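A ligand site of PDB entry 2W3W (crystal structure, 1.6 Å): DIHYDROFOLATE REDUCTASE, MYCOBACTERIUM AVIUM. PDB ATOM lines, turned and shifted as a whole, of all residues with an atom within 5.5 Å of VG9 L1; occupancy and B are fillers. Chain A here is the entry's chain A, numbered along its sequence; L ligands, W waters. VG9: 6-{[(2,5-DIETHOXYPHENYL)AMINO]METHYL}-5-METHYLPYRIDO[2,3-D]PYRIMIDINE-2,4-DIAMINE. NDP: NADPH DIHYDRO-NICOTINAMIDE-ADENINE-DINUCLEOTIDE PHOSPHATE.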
ATOM      1  N   VAL A   9      -7.835 -15.313  17.247  1.00  0.00           N
ATOM      2  CA  VAL A   9      -9.237 -14.988  16.995  1.00  0.00           C
ATOM      3  C   VAL A   9      -9.322 -13.467  16.930  1.00  0.00           C
ATOM      4  O   VAL A   9      -8.869 -12.788  17.826  1.00  0.00           O
ATOM      5  CB  VAL A   9     -10.178 -15.614  18.032  1.00  0.00           C
ATOM      6  CG1 VAL A   9      -9.767 -15.225  19.517  1.00  0.00           C
ATOM      7  CG2 VAL A   9     -11.606 -15.161  17.746  1.00  0.00           C
ATOM      8  N   TRP A  10      -9.864 -12.951  15.828  1.00  0.00           N
ATOM      9  CA  TRP A  10     -10.079 -11.511  15.666  1.00  0.00           C
ATOM     10  C   TRP A  10     -11.268 -11.188  14.783  1.00  0.00           C
ATOM     11  O   TRP A  10     -11.731 -12.061  14.046  1.00  0.00           O
ATOM     12  CB  TRP A  10      -8.814 -10.822  15.108  1.00  0.00           C
ATOM     13  CG  TRP A  10      -8.493 -11.034  13.658  1.00  0.00           C
ATOM     14  CD1 TRP A  10      -8.858 -10.213  12.621  1.00  0.00           C
ATOM     15  CD2 TRP A  10      -7.649 -12.037  13.099  1.00  0.00           C
ATOM     16  NE1 TRP A  10      -8.343 -10.687  11.441  1.00  0.00           N
ATOM     17  CE2 TRP A  10      -7.583 -11.799  11.704  1.00  0.00           C
ATOM     18  CE3 TRP A  10      -6.958 -13.136  13.625  1.00  0.00           C
ATOM     19  CZ2 TRP A  10      -6.820 -12.606  10.839  1.00  0.00           C
ATOM     20  CZ3 TRP A  10      -6.216 -13.948  12.755  1.00  0.00           C
ATOM     21  CH2 TRP A  10      -6.179 -13.683  11.385  1.00  0.00           C
ATOM     22  N   ALA A  11     -11.720  -9.940  14.842  1.00  0.00           N
ATOM     23  CA  ALA A  11     -12.693  -9.339  13.923  1.00  0.00           C
ATOM     24  C   ALA A  11     -12.049  -8.195  13.194  1.00  0.00           C
ATOM     25  O   ALA A  11     -11.368  -7.385  13.786  1.00  0.00           O
ATOM     26  CB  ALA A  11     -13.929  -8.824  14.666  1.00  0.00           C
ATOM     27  N   ILE A  24     -12.578  -0.760  19.559  1.00  0.00           N
ATOM     28  CA  ILE A  24     -13.113  -1.447  18.365  1.00  0.00           C
ATOM     29  C   ILE A  24     -14.171  -0.553  17.724  1.00  0.00           C
ATOM     30  O   ILE A  24     -15.071  -0.052  18.404  1.00  0.00           O
ATOM     31  CB  ILE A  24     -13.652  -2.813  18.731  1.00  0.00           C
ATOM     32  CG1 ILE A  24     -12.487  -3.694  19.214  1.00  0.00           C
ATOM     33  CG2 ILE A  24     -14.343  -3.432  17.522  1.00  0.00           C
ATOM     34  CD1 ILE A  24     -12.874  -4.886  19.943  1.00  0.00           C
ATOM     35  N   ASP A  31     -20.708 -11.098  16.653  1.00  0.00           N
ATOM     36  CA  ASP A  31     -19.276 -11.337  16.726  1.00  0.00           C
ATOM     37  C   ASP A  31     -18.861 -11.522  18.165  1.00  0.00           C
ATOM     38  O   ASP A  31     -18.049 -12.379  18.477  1.00  0.00           O
ATOM     39  CB  ASP A  31     -18.473 -10.198  16.136  1.00  0.00           C
ATOM     40  CG  ASP A  31     -16.959 -10.345  16.419  1.00  0.00           C
ATOM     41  OD1 ASP A  31     -16.361 -11.330  15.921  1.00  0.00           O
ATOM     42  OD2 ASP A  31     -16.387  -9.492  17.125  1.00  0.00           O
ATOM     43  N   LEU A  32     -19.414 -10.709  19.060  1.00  0.00           N
ATOM     44  CA  LEU A  32     -19.097 -10.904  20.466  1.00  0.00           C
ATOM     45  C   LEU A  32     -19.538 -12.299  20.924  1.00  0.00           C
ATOM     46  O   LEU A  32     -18.844 -12.971  21.687  1.00  0.00           O
ATOM     47  CB  LEU A  32     -19.744  -9.824  21.317  1.00  0.00           C
ATOM     48  CG  LEU A  32     -19.193  -9.765  22.738  1.00  0.00           C
ATOM     49  CD1 LEU A  32     -17.743  -9.352  22.768  1.00  0.00           C
ATOM     50  CD2 LEU A  32     -20.048  -8.830  23.567  1.00  0.00           C
ATOM     51  N   PHE A  35     -16.946 -14.749  19.648  1.00  0.00           N
ATOM     52  CA  PHE A  35     -15.728 -14.623  20.421  1.00  0.00           C
ATOM     53  C   PHE A  35     -15.843 -15.310  21.773  1.00  0.00           C
ATOM     54  O   PHE A  35     -14.927 -15.996  22.206  1.00  0.00           O
ATOM     55  CB  PHE A  35     -15.417 -13.158  20.668  1.00  0.00           C
ATOM     56  CG  PHE A  35     -14.322 -12.944  21.634  1.00  0.00           C
ATOM     57  CD1 PHE A  35     -13.019 -13.279  21.300  1.00  0.00           C
ATOM     58  CD2 PHE A  35     -14.569 -12.347  22.867  1.00  0.00           C
ATOM     59  CE1 PHE A  35     -11.994 -13.067  22.173  1.00  0.00           C
ATOM     60  CE2 PHE A  35     -13.532 -12.115  23.748  1.00  0.00           C
ATOM     61  CZ  PHE A  35     -12.253 -12.477  23.405  1.00  0.00           C
ATOM     62  N   LYS A  36     -16.958 -15.097  22.457  1.00  0.00           N
ATOM     63  CA  LYS A  36     -17.240 -15.778  23.712  1.00  0.00           C
ATOM     64  C   LYS A  36     -17.255 -17.286  23.533  1.00  0.00           C
ATOM     65  O   LYS A  36     -16.683 -18.004  24.348  1.00  0.00           O
ATOM     66  CB  LYS A  36     -18.557 -15.317  24.310  1.00  0.00           C
ATOM     67  CG  LYS A  36     -18.556 -13.934  24.868  1.00  0.00           C
ATOM     68  CD  LYS A  36     -19.962 -13.539  25.311  1.00  0.00           C
ATOM     69  CE  LYS A  36     -20.088 -12.043  25.477  1.00  0.00           C
ATOM     70  NZ  LYS A  36     -21.424 -11.651  26.037  1.00  0.00           N
ATOM     71  N   THR A  50      -4.387  -4.221  24.595  1.00  0.00           N
ATOM     72  CA  THR A  50      -5.705  -4.873  24.511  1.00  0.00           C
ATOM     73  C   THR A  50      -6.305  -5.061  25.906  1.00  0.00           C
ATOM     74  O   THR A  50      -7.457  -4.673  26.173  1.00  0.00           O
ATOM     75  CB  THR A  50      -5.648  -6.155  23.744  1.00  0.00           C
ATOM     76  OG1 THR A  50      -5.320  -5.820  22.375  1.00  0.00           O
ATOM     77  CG2 THR A  50      -6.998  -6.905  23.786  1.00  0.00           C
ATOM     78  N   LEU A  54     -10.010  -3.383  27.307  1.00  0.00           N
ATOM     79  CA  LEU A  54     -11.219  -4.131  27.660  1.00  0.00           C
ATOM     80  C   LEU A  54     -12.126  -3.296  28.585  1.00  0.00           C
ATOM     81  O   LEU A  54     -11.654  -2.540  29.425  1.00  0.00           O
ATOM     82  CB  LEU A  54     -10.878  -5.456  28.344  1.00  0.00           C
ATOM     83  CG  LEU A  54     -10.104  -6.502  27.572  1.00  0.00           C
ATOM     84  CD1 LEU A  54      -9.784  -7.648  28.510  1.00  0.00           C
ATOM     85  CD2 LEU A  54     -10.860  -7.015  26.357  1.00  0.00           C
ATOM     86  N   PRO A  55     -13.444  -3.414  28.393  1.00  0.00           N
ATOM     87  CA  PRO A  55     -14.336  -2.782  29.342  1.00  0.00           C
ATOM     88  C   PRO A  55     -14.086  -3.354  30.752  1.00  0.00           C
ATOM     89  O   PRO A  55     -13.871  -4.574  30.888  1.00  0.00           O
ATOM     90  CB  PRO A  55     -15.725  -3.163  28.838  1.00  0.00           C
ATOM     91  CG  PRO A  55     -15.578  -3.600  27.475  1.00  0.00           C
ATOM     92  CD  PRO A  55     -14.180  -4.113  27.322  1.00  0.00           C
ATOM     93  N   VAL A  58     -15.744  -6.536  32.135  1.00  0.00           N
ATOM     94  CA  VAL A  58     -15.348  -7.868  31.636  1.00  0.00           C
ATOM     95  C   VAL A  58     -13.836  -8.094  31.733  1.00  0.00           C
ATOM     96  O   VAL A  58     -13.268  -8.831  30.941  1.00  0.00           O
ATOM     97  CB  VAL A  58     -15.775  -8.087  30.162  1.00  0.00           C
ATOM     98  CG1 VAL A  58     -17.312  -8.020  30.046  1.00  0.00           C
ATOM     99  CG2 VAL A  58     -15.089  -7.075  29.226  1.00  0.00           C
ATOM    100  N   LEU A  61     -11.419 -11.416  31.811  1.00  0.00           N
ATOM    101  CA  LEU A  61     -12.516 -12.135  31.145  1.00  0.00           C
ATOM    102  C   LEU A  61     -12.891 -13.376  31.953  1.00  0.00           C
ATOM    103  O   LEU A  61     -12.035 -14.195  32.255  1.00  0.00           O
ATOM    104  CB  LEU A  61     -12.088 -12.509  29.704  1.00  0.00           C
ATOM    105  CG  LEU A  61     -11.730 -11.323  28.786  1.00  0.00           C
ATOM    106  CD1 LEU A  61     -11.023 -11.787  27.503  1.00  0.00           C
ATOM    107  CD2 LEU A  61     -12.942 -10.485  28.414  1.00  0.00           C
ATOM    108  N   PRO A  62     -14.176 -13.527  32.349  1.00  0.00           N
ATOM    109  CA  PRO A  62     -14.523 -14.621  33.260  1.00  0.00           C
ATOM    110  C   PRO A  62     -14.449 -16.031  32.648  1.00  0.00           C
ATOM    111  O   PRO A  62     -14.756 -16.211  31.474  1.00  0.00           O
ATOM    112  CB  PRO A  62     -15.945 -14.302  33.679  1.00  0.00           C
ATOM    113  CG  PRO A  62     -16.490 -13.465  32.605  1.00  0.00           C
ATOM    114  CD  PRO A  62     -15.363 -12.717  31.985  1.00  0.00           C
ATOM    115  N   ARG A  64     -11.945 -17.822  31.897  1.00  0.00           N
ATOM    116  CA  ARG A  64     -10.799 -17.993  31.039  1.00  0.00           C
ATOM    117  C   ARG A  64      -9.564 -17.588  31.827  1.00  0.00           C
ATOM    118  O   ARG A  64      -9.638 -16.700  32.677  1.00  0.00           O
ATOM    119  CB  ARG A  64     -10.942 -17.063  29.852  1.00  0.00           C
ATOM    120  CG  ARG A  64     -12.109 -17.360  28.935  1.00  0.00           C
ATOM    121  CD  ARG A  64     -12.602 -16.115  28.258  1.00  0.00           C
ATOM    122  NE  ARG A  64     -13.803 -16.375  27.485  1.00  0.00           N
ATOM    123  CZ  ARG A  64     -15.046 -16.075  27.843  1.00  0.00           C
ATOM    124  NH1 ARG A  64     -15.342 -15.461  28.995  1.00  0.00           N
ATOM    125  NH2 ARG A  64     -16.031 -16.403  27.028  1.00  0.00           N
ATOM    126  N   VAL A 101      -5.010 -16.614  21.226  1.00  0.00           N
ATOM    127  CA  VAL A 101      -4.488 -15.242  21.202  1.00  0.00           C
ATOM    128  C   VAL A 101      -5.605 -14.302  20.714  1.00  0.00           C
ATOM    129  O   VAL A 101      -6.188 -14.490  19.633  1.00  0.00           O
ATOM    130  CB  VAL A 101      -3.246 -15.163  20.342  1.00  0.00           C
ATOM    131  CG1 VAL A 101      -2.756 -13.693  20.236  1.00  0.00           C
ATOM    132  CG2 VAL A 101      -2.112 -16.086  20.875  1.00  0.00           C
ATOM    133  N   ILE A 102      -5.930 -13.317  21.549  1.00  0.00           N
ATOM    134  CA  ILE A 102      -7.106 -12.496  21.365  1.00  0.00           C
ATOM    135  C   ILE A 102      -6.795 -11.005  20.994  1.00  0.00           C
ATOM    136  O   ILE A 102      -7.696 -10.196  20.938  1.00  0.00           O
ATOM    137  CB  ILE A 102      -8.080 -12.599  22.591  1.00  0.00           C
ATOM    138  CG1 ILE A 102      -7.518 -11.859  23.820  1.00  0.00           C
ATOM    139  CG2 ILE A 102      -8.514 -14.067  22.897  1.00  0.00           C
ATOM    140  CD1 ILE A 102      -8.531 -11.599  24.897  1.00  0.00           C
ATOM    141  N   GLY A 103      -5.521 -10.689  20.724  1.00  0.00           N
ATOM    142  CA  GLY A 103      -5.128  -9.399  20.175  1.00  0.00           C
ATOM    143  C   GLY A 103      -4.113  -8.711  21.037  1.00  0.00           C
ATOM    144  O   GLY A 103      -3.800  -9.205  22.114  1.00  0.00           O
ATOM    145  N   TYR A 108      -0.735 -10.278  17.636  1.00  0.00           N
ATOM    146  CA  TYR A 108      -1.051 -11.232  16.554  1.00  0.00           C
ATOM    147  C   TYR A 108       0.191 -11.546  15.716  1.00  0.00           C
ATOM    148  O   TYR A 108       0.429 -12.718  15.393  1.00  0.00           O
ATOM    149  CB  TYR A 108      -2.151 -10.758  15.613  1.00  0.00           C
ATOM    150  CG  TYR A 108      -3.555 -10.740  16.230  1.00  0.00           C
ATOM    151  CD1 TYR A 108      -4.077 -11.833  16.884  1.00  0.00           C
ATOM    152  CD2 TYR A 108      -4.353  -9.623  16.109  1.00  0.00           C
ATOM    153  CE1 TYR A 108      -5.341 -11.798  17.445  1.00  0.00           C
ATOM    154  CE2 TYR A 108      -5.624  -9.564  16.670  1.00  0.00           C
ATOM    155  CZ  TYR A 108      -6.128 -10.665  17.356  1.00  0.00           C
ATOM    156  OH  TYR A 108      -7.396 -10.597  17.914  1.00  0.00           O
ATOM    157  N   GLU A 119      -9.592 -17.968  13.717  1.00  0.00           N
ATOM    158  CA  GLU A 119     -11.036 -17.749  13.636  1.00  0.00           C
ATOM    159  C   GLU A 119     -11.256 -16.276  13.426  1.00  0.00           C
ATOM    160  O   GLU A 119     -11.001 -15.469  14.326  1.00  0.00           O
ATOM    161  CB  GLU A 119     -11.751 -18.260  14.894  1.00  0.00           C
ATOM    162  CG  GLU A 119     -11.698 -19.773  15.035  1.00  0.00           C
ATOM    163  CD  GLU A 119     -12.456 -20.567  13.946  1.00  0.00           C
ATOM    164  OE1 GLU A 119     -13.453 -20.101  13.396  1.00  0.00           O
ATOM    165  OE2 GLU A 119     -12.013 -21.676  13.617  1.00  0.00           O
ATOM    166  N   THR A 121     -13.656 -12.991  12.037  1.00  0.00           N
ATOM    167  CA  THR A 121     -14.928 -12.406  11.612  1.00  0.00           C
ATOM    168  C   THR A 121     -14.649 -11.241  10.685  1.00  0.00           C
ATOM    169  O   THR A 121     -13.812 -10.396  11.017  1.00  0.00           O
ATOM    170  CB  THR A 121     -15.719 -11.896  12.803  1.00  0.00           C
ATOM    171  OG1 THR A 121     -15.850 -12.932  13.782  1.00  0.00           O
ATOM    172  CG2 THR A 121     -17.111 -11.361  12.375  1.00  0.00           C
HETATM  173  N2  VG9 L   1     -13.786 -11.896  16.930  1.00  0.00           N
HETATM  174  C2  VG9 L   1     -13.281 -11.179  17.955  1.00  0.00           C
HETATM  175  N3  VG9 L   1     -12.061 -11.474  18.478  1.00  0.00           N
HETATM  176  C4  VG9 L   1     -11.550 -10.780  19.503  1.00  0.00           C
HETATM  177  N4  VG9 L   1     -10.294 -11.128  19.822  1.00  0.00           N
HETATM  178  N1  VG9 L   1     -14.022 -10.169  18.458  1.00  0.00           N
HETATM  179  C8A VG9 L   1     -13.582  -9.494  19.532  1.00  0.00           C
HETATM  180  N8  VG9 L   1     -14.385  -8.543  20.023  1.00  0.00           N
HETATM  181  C7  VG9 L   1     -14.021  -7.814  21.093  1.00  0.00           C
HETATM  182  C6  VG9 L   1     -12.810  -7.998  21.742  1.00  0.00           C
HETATM  183  C5  VG9 L   1     -11.946  -8.992  21.243  1.00  0.00           C
HETATM  184  C5A VG9 L   1     -10.652  -9.217  21.960  1.00  0.00           C
HETATM  185  C4A VG9 L   1     -12.333  -9.752  20.109  1.00  0.00           C
HETATM  186  C9  VG9 L   1     -12.445  -7.125  22.951  1.00  0.00           C
HETATM  187  N10 VG9 L   1     -13.637  -6.466  23.509  1.00  0.00           N
HETATM  188  C11 VG9 L   1     -14.641  -7.076  24.190  1.00  0.00           C
HETATM  189  C12 VG9 L   1     -15.806  -6.353  24.442  1.00  0.00           C
HETATM  190  O2  VG9 L   1     -15.922  -5.049  23.994  1.00  0.00           O
HETATM  191  C13 VG9 L   1     -16.865  -6.927  25.112  1.00  0.00           C
HETATM  192  C14 VG9 L   1     -16.783  -8.223  25.589  1.00  0.00           C
HETATM  193  C15 VG9 L   1     -15.653  -8.973  25.357  1.00  0.00           C
HETATM  194  C16 VG9 L   1     -14.582  -8.400  24.658  1.00  0.00           C
HETATM  195  O5  VG9 L   1     -15.559 -10.270  25.806  1.00  0.00           O
HETATM  196  C51 VG9 L   1     -16.538 -10.900  26.650  1.00  0.00           C
HETATM  197  C52 VG9 L   1     -16.059 -12.271  27.075  1.00  0.00           C
HETATM  198  PA  NDP L   2      -1.504  -4.952  21.615  1.00  0.00           P
HETATM  199  O1A NDP L   2      -0.950  -5.861  20.599  1.00  0.00           O
HETATM  200  O2A NDP L   2      -2.758  -5.363  22.300  1.00  0.00           O
HETATM  201  O5B NDP L   2      -0.467  -4.594  22.777  1.00  0.00           O
HETATM  202  C5B NDP L   2       0.804  -4.125  22.382  1.00  0.00           C
HETATM  203  C4B NDP L   2       1.708  -4.173  23.611  1.00  0.00           C
HETATM  204  O4B NDP L   2       2.118  -5.530  23.746  1.00  0.00           O
HETATM  205  C3B NDP L   2       3.005  -3.356  23.593  1.00  0.00           C
HETATM  206  O3B NDP L   2       2.693  -2.014  23.984  1.00  0.00           O
HETATM  207  C2B NDP L   2       3.776  -4.145  24.631  1.00  0.00           C
HETATM  208  O2B NDP L   2       3.358  -3.869  25.954  1.00  0.00           O
HETATM  209  C1B NDP L   2       3.389  -5.605  24.308  1.00  0.00           C
HETATM  210  N9A NDP L   2       4.335  -6.201  23.354  1.00  0.00           N
HETATM  211  C8A NDP L   2       4.403  -6.004  22.009  1.00  0.00           C
HETATM  212  N7A NDP L   2       5.435  -6.716  21.512  1.00  0.00           N
HETATM  213  C5A NDP L   2       6.020  -7.368  22.556  1.00  0.00           C
HETATM  214  C6A NDP L   2       7.087  -8.222  22.644  1.00  0.00           C
HETATM  215  N6A NDP L   2       7.828  -8.458  21.537  1.00  0.00           N
HETATM  216  N1A NDP L   2       7.449  -8.741  23.849  1.00  0.00           N
HETATM  217  C2A NDP L   2       6.744  -8.423  24.984  1.00  0.00           C
HETATM  218  N3A NDP L   2       5.671  -7.558  24.890  1.00  0.00           N
HETATM  219  C4A NDP L   2       5.327  -7.060  23.710  1.00  0.00           C
HETATM  220  O3  NDP L   2      -1.771  -3.460  21.043  1.00  0.00           O
HETATM  221  PN  NDP L   2      -2.177  -2.900  19.603  1.00  0.00           P
HETATM  222  O1N NDP L   2      -1.365  -3.443  18.523  1.00  0.00           O
HETATM  223  O2N NDP L   2      -2.231  -1.397  19.759  1.00  0.00           O
HETATM  224  O5D NDP L   2      -3.703  -3.363  19.497  1.00  0.00           O
HETATM  225  C5D NDP L   2      -4.768  -2.942  20.337  1.00  0.00           C
HETATM  226  C4D NDP L   2      -5.901  -2.417  19.467  1.00  0.00           C
HETATM  227  O4D NDP L   2      -6.537  -3.562  18.846  1.00  0.00           O
HETATM  228  C3D NDP L   2      -7.042  -1.695  20.167  1.00  0.00           C
HETATM  229  O3D NDP L   2      -7.578  -0.726  19.284  1.00  0.00           O
HETATM  230  C2D NDP L   2      -8.099  -2.773  20.427  1.00  0.00           C
HETATM  231  O2D NDP L   2      -9.369  -2.259  20.617  1.00  0.00           O
HETATM  232  C1D NDP L   2      -7.918  -3.566  19.152  1.00  0.00           C
HETATM  233  N1N NDP L   2      -8.404  -4.954  19.286  1.00  0.00           N
HETATM  234  C2N NDP L   2      -9.208  -5.415  18.304  1.00  0.00           C
HETATM  235  C3N NDP L   2      -9.660  -6.712  18.327  1.00  0.00           C
HETATM  236  C7N NDP L   2     -10.479  -7.172  17.204  1.00  0.00           C
HETATM  237  O7N NDP L   2     -10.607  -8.508  17.055  1.00  0.00           O
HETATM  238  N7N NDP L   2     -11.066  -6.310  16.386  1.00  0.00           N
HETATM  239  C4N NDP L   2      -9.093  -7.750  19.235  1.00  0.00           C
HETATM  240  C5N NDP L   2      -8.213  -7.146  20.237  1.00  0.00           C
HETATM  241  C6N NDP L   2      -7.886  -5.810  20.211  1.00  0.00           C
HETATM  242  P2B NDP L   2       4.229  -2.828  26.926  1.00  0.00           P
HETATM  243  O1X NDP L   2       4.063  -1.536  26.160  1.00  0.00           O
HETATM  244  O2X NDP L   2       3.533  -2.881  28.224  1.00  0.00           O
HETATM  245  O3X NDP L   2       5.653  -3.285  26.941  1.00  0.00           O
HETATM  246  O   HOH W   1     -16.371  -7.019  17.871  1.00  0.00           O
HETATM  247  O   HOH W   2     -13.795 -14.309  14.990  1.00  0.00           O
HETATM  248  O   HOH W   3     -13.049  -3.359  23.554  1.00  0.00           O
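The backbone carbonyl oxygen (O) of Ala 11 sits at hydrogen-bond distance from a nitrogen (N7N) of NDP L2 (2.8 Å).
The side-chain carboxylate of Asp 31 is in hydrogen-bond range of a nitrogen (N1) of VG9 L1, 2.8 Å away.
The side-chain hydroxyl (OG1) of Thr 50 sits at hydrogen-bond distance from an oxygen (O2A) of NDP L2, 2.6 Å away.
An oxygen (O7N) of NDP L2 sits at hydrogen-bond distance from the backbone NH (N) of Ala 11, 2.9 Å away.
N4 of VG9 L1 is in hydrogen-bond range of O of Ile 102.
N of Thr 50 lies within hydrogen-bond range of O2A of NDP L2 (3.0 Å).
A nitrogen (N4) of VG9 L1 is in hydrogen-bond range of the backbone carbonyl oxygen (O) of Val 9.
OD1 of Asp 31 lies within hydrogen-bond range of OG1 of Thr 121 (2.7 Å).
OH of Tyr 108 is in hydrogen-bond range of O of Val 9, 2.6 Å away.
O of Val 101 lies within hydrogen-bond range of N of Val 9 (3.0 Å).
The backbone carbonyl oxygen of Lys 36 lies within hydrogen-bond range of the guanidinium group of Arg 64.
The backbone NH (N) of Thr 121 lies within hydrogen-bond range of the backbone carbonyl oxygen (O) of Trp 10 (2.9 Å).
O of Pro 62 sits at hydrogen-bond distance from NH1 of Arg 64 (2.7 Å).
N of Gly 103 sits at hydrogen-bond distance from OH of Tyr 108 (3.4 Å).
The side-chain hydroxyl (OH) of Tyr 108 lies within hydrogen-bond range of the backbone carbonyl oxygen (O) of Ile 102, 3.1 Å away.
C of Trp 10 touches N2 of VG9 L1, at 3.4 Å.
Ala 11 touches VG9 L1 (N to N2, 3.5 Å).
Ile 24 touches VG9 L1 (CD1 to C7, 3.3 Å).
CD1 of Leu 32 touches C14 of VG9 L1, 3.2 Å away.
CD1 of Phe 35 touches C4 of VG9 L1, 3.4 Å away.
CG of Lys 36 touches C52 of VG9 L1 (3.7 Å).
Leu 54 touches VG9 L1 (CD2 to C9, 3.8 Å).
Pro 55 touches VG9 L1 (CG to O2, 3.8 Å).
CD2 of Leu 61 touches O5 of VG9 L1, 3.7 Å away.
NH1 of Arg 64 touches C52 of VG9 L1 (3.8 Å).
OH of Tyr 108 touches N4 of VG9 L1 (3.5 Å).
Thr 121 touches VG9 L1.
Within 4 Å of VG9 L1: Val 9, Trp 10, Ala 11, Ile 24, Asp 31, Leu 32, Phe 35, Lys 36, Leu 54, Pro 55, Leu 61, Arg 64, Ile 102, Tyr 108 and Thr 121.
Water W2 lies within hydrogen-bond range of the side-chain hydroxyl of Thr 121 (2.8 Å), a nitrogen (N2) of VG9 L1 (3.1 Å), the backbone carbonyl oxygen of Glu 119 (3.1 Å) and the backbone carbonyl oxygen of Trp 10 (3.2 Å).
Water W1 bridges the side-chain carboxylate (OD2) of Asp 31 (2.6 Å) and a nitrogen (N8) of VG9 L1 (3.3 Å).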
